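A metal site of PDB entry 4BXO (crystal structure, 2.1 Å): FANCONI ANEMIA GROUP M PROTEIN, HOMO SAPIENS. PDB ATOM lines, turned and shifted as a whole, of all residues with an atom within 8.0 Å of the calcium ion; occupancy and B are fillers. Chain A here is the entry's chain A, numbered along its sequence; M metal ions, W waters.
The calcium ion is bound by water W1 (2.2 Å), the side-chain carboxylate (OD2) of Asp 60 (2.2 Å), the backbone carbonyl oxygen (O) of Arg 71 (2.3 Å) and the side-chain carboxylate (OE2) of Glu 70 (2.7 Å).
OE2 of Glu 70 lies close to NH1 of Arg 72 (3.0 Å).
The side-chain carboxylate (OD1) of Asp 60 is in hydrogen-bond range of a ring nitrogen (NE2) of His 31 (2.7 Å).
NH1 of Arg 71 is in salt-bridge range of OE1 of Glu 32.
OE1 of Glu 70 is in hydrogen-bond range of NE2 of Gln 89.
The backbone NH (N) of Ile 103 sits at hydrogen-bond distance from the backbone carbonyl oxygen (O) of Glu 70, at 2.9 Å.
The backbone carbonyl oxygen (O) of Ser 35 is in hydrogen-bond range of the guanidinium group (NH2) of Arg 71, at 3.1 Å.
Within 4 Å of the calcium ion: Asp 60, Glu 70 and Arg 71.
The nearest printed residue that does not touch the calcium ion is Glu 32 (4.3 Å).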
ATOM      1  N   HIS A  31       6.762 -21.734   0.130  1.00  0.00           N
ATOM      2  CA  HIS A  31       8.184 -21.970   0.173  1.00  0.00           C
ATOM      3  C   HIS A  31       8.993 -20.642   0.078  1.00  0.00           C
ATOM      4  O   HIS A  31      10.122 -20.605   0.550  1.00  0.00           O
ATOM      5  CB  HIS A  31       8.597 -22.928  -0.956  1.00  0.00           C
ATOM      6  CG  HIS A  31       8.300 -22.408  -2.316  1.00  0.00           C
ATOM      7  ND1 HIS A  31       7.052 -22.530  -2.895  1.00  0.00           N
ATOM      8  CD2 HIS A  31       9.065 -21.730  -3.208  1.00  0.00           C
ATOM      9  CE1 HIS A  31       7.073 -21.976  -4.084  1.00  0.00           C
ATOM     10  NE2 HIS A  31       8.293 -21.489  -4.309  1.00  0.00           N
ATOM     11  N   GLU A  32       8.411 -19.595  -0.518  1.00  0.00           N
ATOM     12  CA  GLU A  32       9.015 -18.238  -0.563  1.00  0.00           C
ATOM     13  C   GLU A  32       9.092 -17.546   0.831  1.00  0.00           C
ATOM     14  O   GLU A  32       9.775 -16.549   0.991  1.00  0.00           O
ATOM     15  CB  GLU A  32       8.300 -17.263  -1.539  1.00  0.00           C
ATOM     16  CG  GLU A  32       8.413 -17.622  -2.938  1.00  0.00           C
ATOM     17  CD  GLU A  32       9.842 -17.528  -3.444  1.00  0.00           C
ATOM     18  OE1 GLU A  32      10.372 -16.404  -3.538  1.00  0.00           O
ATOM     19  OE2 GLU A  32      10.417 -18.622  -3.739  1.00  0.00           O
ATOM     20  N   SER A  35      12.816 -18.469   1.333  1.00  0.00           N
ATOM     21  CA  SER A  35      13.783 -17.925   0.338  1.00  0.00           C
ATOM     22  C   SER A  35      13.508 -16.462   0.029  1.00  0.00           C
ATOM     23  O   SER A  35      14.449 -15.722  -0.283  1.00  0.00           O
ATOM     24  CB  SER A  35      13.791 -18.768  -0.954  1.00  0.00           C
ATOM     25  OG  SER A  35      12.474 -19.034  -1.500  1.00  0.00           O
ATOM     26  N   GLY A  58       5.732 -25.695  -5.788  1.00  0.00           N
ATOM     27  CA  GLY A  58       6.698 -25.284  -6.820  1.00  0.00           C
ATOM     28  C   GLY A  58       6.563 -23.850  -7.335  1.00  0.00           C
ATOM     29  O   GLY A  58       7.619 -23.131  -7.518  1.00  0.00           O
ATOM     30  N   CYS A  59       5.330 -23.357  -7.539  1.00  0.00           N
ATOM     31  CA  CYS A  59       5.184 -22.036  -8.096  1.00  0.00           C
ATOM     32  C   CYS A  59       5.537 -20.910  -7.090  1.00  0.00           C
ATOM     33  O   CYS A  59       4.913 -20.790  -6.011  1.00  0.00           O
ATOM     34  CB  CYS A  59       3.810 -21.809  -8.739  1.00  0.00           C
ATOM     35  SG  CYS A  59       3.307 -23.150  -9.712  1.00  0.00           S
ATOM     36  N   ASP A  60       6.464 -20.043  -7.517  1.00  0.00           N
ATOM     37  CA  ASP A  60       6.905 -18.962  -6.674  1.00  0.00           C
ATOM     38  C   ASP A  60       5.823 -17.897  -6.559  1.00  0.00           C
ATOM     39  O   ASP A  60       5.419 -17.577  -5.457  1.00  0.00           O
ATOM     40  CB  ASP A  60       8.251 -18.367  -7.092  1.00  0.00           C
ATOM     41  CG  ASP A  60       9.352 -19.379  -7.127  1.00  0.00           C
ATOM     42  OD1 ASP A  60       9.237 -20.467  -6.581  1.00  0.00           O
ATOM     43  OD2 ASP A  60      10.389 -19.025  -7.687  1.00  0.00           O
ATOM     44  N   TYR A  61       5.427 -17.310  -7.685  1.00  0.00           N
ATOM     45  CA  TYR A  61       4.400 -16.282  -7.695  1.00  0.00           C
ATOM     46  C   TYR A  61       3.358 -16.510  -8.816  1.00  0.00           C
ATOM     47  O   TYR A  61       3.723 -16.798  -9.954  1.00  0.00           O
ATOM     48  CB  TYR A  61       4.987 -14.856  -7.778  1.00  0.00           C
ATOM     49  CG  TYR A  61       5.982 -14.642  -6.668  1.00  0.00           C
ATOM     50  CD1 TYR A  61       7.284 -15.123  -6.777  1.00  0.00           C
ATOM     51  CD2 TYR A  61       5.588 -14.021  -5.436  1.00  0.00           C
ATOM     52  CE1 TYR A  61       8.220 -14.960  -5.697  1.00  0.00           C
ATOM     53  CE2 TYR A  61       6.493 -13.876  -4.377  1.00  0.00           C
ATOM     54  CZ  TYR A  61       7.777 -14.382  -4.484  1.00  0.00           C
ATOM     55  OH  TYR A  61       8.691 -14.267  -3.455  1.00  0.00           O
ATOM     56  N   VAL A  69       5.441 -16.669 -12.251  1.00  0.00           N
ATOM     57  CA  VAL A  69       6.776 -16.082 -12.194  1.00  0.00           C
ATOM     58  C   VAL A  69       7.664 -17.029 -11.435  1.00  0.00           C
ATOM     59  O   VAL A  69       7.316 -17.494 -10.336  1.00  0.00           O
ATOM     60  CB  VAL A  69       6.778 -14.690 -11.558  1.00  0.00           C
ATOM     61  CG1 VAL A  69       8.168 -14.083 -11.594  1.00  0.00           C
ATOM     62  CG2 VAL A  69       5.840 -13.767 -12.270  1.00  0.00           C
ATOM     63  N   GLU A  70       8.795 -17.343 -12.029  1.00  0.00           N
ATOM     64  CA  GLU A  70       9.813 -18.095 -11.364  1.00  0.00           C
ATOM     65  C   GLU A  70      10.930 -17.161 -10.984  1.00  0.00           C
ATOM     66  O   GLU A  70      11.553 -16.522 -11.814  1.00  0.00           O
ATOM     67  CB  GLU A  70      10.362 -19.177 -12.287  1.00  0.00           C
ATOM     68  CG  GLU A  70      11.397 -20.064 -11.687  1.00  0.00           C
ATOM     69  CD  GLU A  70      10.880 -20.937 -10.574  1.00  0.00           C
ATOM     70  OE1 GLU A  70       9.717 -21.393 -10.575  1.00  0.00           O
ATOM     71  OE2 GLU A  70      11.676 -21.186  -9.640  1.00  0.00           O
ATOM     72  N   ARG A  71      11.160 -17.075  -9.690  1.00  0.00           N
ATOM     73  CA  ARG A  71      12.257 -16.326  -9.166  1.00  0.00           C
ATOM     74  C   ARG A  71      13.473 -17.255  -9.060  1.00  0.00           C
ATOM     75  O   ARG A  71      13.396 -18.302  -8.532  1.00  0.00           O
ATOM     76  CB  ARG A  71      11.854 -15.798  -7.796  1.00  0.00           C
ATOM     77  CG  ARG A  71      12.852 -15.011  -7.062  1.00  0.00           C
ATOM     78  CD  ARG A  71      12.267 -14.528  -5.743  1.00  0.00           C
ATOM     79  NE  ARG A  71      13.337 -14.110  -4.853  1.00  0.00           N
ATOM     80  CZ  ARG A  71      13.630 -14.729  -3.719  1.00  0.00           C
ATOM     81  NH1 ARG A  71      12.936 -15.778  -3.326  1.00  0.00           N
ATOM     82  NH2 ARG A  71      14.631 -14.287  -3.001  1.00  0.00           N
ATOM     83  N   ARG A  72      14.609 -16.825  -9.596  1.00  0.00           N
ATOM     84  CA  ARG A  72      15.814 -17.661  -9.642  1.00  0.00           C
ATOM     85  C   ARG A  72      17.030 -16.820  -9.276  1.00  0.00           C
ATOM     86  O   ARG A  72      17.171 -15.670  -9.770  1.00  0.00           O
ATOM     87  CB  ARG A  72      15.917 -18.217 -11.066  1.00  0.00           C
ATOM     88  CG  ARG A  72      16.363 -19.637 -11.153  1.00  0.00           C
ATOM     89  CD  ARG A  72      15.295 -20.627 -10.831  1.00  0.00           C
ATOM     90  NE  ARG A  72      15.923 -21.916 -10.565  1.00  0.00           N
ATOM     91  CZ  ARG A  72      15.268 -23.045 -10.267  1.00  0.00           C
ATOM     92  NH1 ARG A  72      13.926 -23.123 -10.200  1.00  0.00           N
ATOM     93  NH2 ARG A  72      15.958 -24.111 -10.041  1.00  0.00           N
ATOM     94  N   SER A  73      17.912 -17.360  -8.441  1.00  0.00           N
ATOM     95  CA  SER A  73      19.143 -16.646  -8.129  1.00  0.00           C
ATOM     96  C   SER A  73      20.106 -16.688  -9.288  1.00  0.00           C
ATOM     97  O   SER A  73      20.162 -17.654 -10.038  1.00  0.00           O
ATOM     98  CB  SER A  73      19.806 -17.093  -6.823  1.00  0.00           C
ATOM     99  OG  SER A  73      20.794 -18.025  -7.065  1.00  0.00           O
ATOM    100  N   PHE A  86      16.557 -26.599 -13.789  1.00  0.00           N
ATOM    101  CA  PHE A  86      15.860 -25.370 -14.134  1.00  0.00           C
ATOM    102  C   PHE A  86      14.931 -25.585 -15.332  1.00  0.00           C
ATOM    103  O   PHE A  86      13.794 -25.092 -15.314  1.00  0.00           O
ATOM    104  CB  PHE A  86      16.860 -24.261 -14.442  1.00  0.00           C
ATOM    105  CG  PHE A  86      16.238 -23.006 -14.871  1.00  0.00           C
ATOM    106  CD1 PHE A  86      15.689 -22.139 -13.967  1.00  0.00           C
ATOM    107  CD2 PHE A  86      16.124 -22.691 -16.218  1.00  0.00           C
ATOM    108  CE1 PHE A  86      15.064 -20.942 -14.395  1.00  0.00           C
ATOM    109  CE2 PHE A  86      15.548 -21.499 -16.625  1.00  0.00           C
ATOM    110  CZ  PHE A  86      14.992 -20.638 -15.710  1.00  0.00           C
ATOM    111  N   GLN A  89      11.847 -27.580 -14.217  1.00  0.00           N
ATOM    112  CA  GLN A  89      10.913 -26.711 -13.545  1.00  0.00           C
ATOM    113  C   GLN A  89      10.120 -25.832 -14.579  1.00  0.00           C
ATOM    114  O   GLN A  89       8.888 -25.712 -14.469  1.00  0.00           O
ATOM    115  CB  GLN A  89      11.609 -25.895 -12.479  1.00  0.00           C
ATOM    116  CG  GLN A  89      10.764 -24.761 -11.842  1.00  0.00           C
ATOM    117  CD  GLN A  89       9.588 -25.253 -10.965  1.00  0.00           C
ATOM    118  OE1 GLN A  89       9.464 -26.426 -10.698  1.00  0.00           O
ATOM    119  NE2 GLN A  89       8.718 -24.330 -10.558  1.00  0.00           N
ATOM    120  N   ILE A 103      12.295 -14.069 -13.179  1.00  0.00           N
ATOM    121  CA  ILE A 103      13.025 -13.011 -12.618  1.00  0.00           C
ATOM    122  C   ILE A 103      14.414 -13.536 -12.143  1.00  0.00           C
ATOM    123  O   ILE A 103      14.474 -14.367 -11.272  1.00  0.00           O
ATOM    124  CB  ILE A 103      12.235 -12.277 -11.479  1.00  0.00           C
ATOM    125  CG1 ILE A 103      10.936 -11.656 -12.029  1.00  0.00           C
ATOM    126  CG2 ILE A 103      13.100 -11.297 -10.808  1.00  0.00           C
ATOM    127  CD1 ILE A 103      10.038 -11.109 -10.991  1.00  0.00           C
HETATM  128 CA    CA M   1      12.363 -20.025  -7.330  1.00  0.00          CA
HETATM  129  O   HOH W   1      14.390 -20.802  -7.082  1.00  0.00           O
HETATM  130  O   HOH W   2      10.132 -22.366  -7.841  1.00  0.00           O
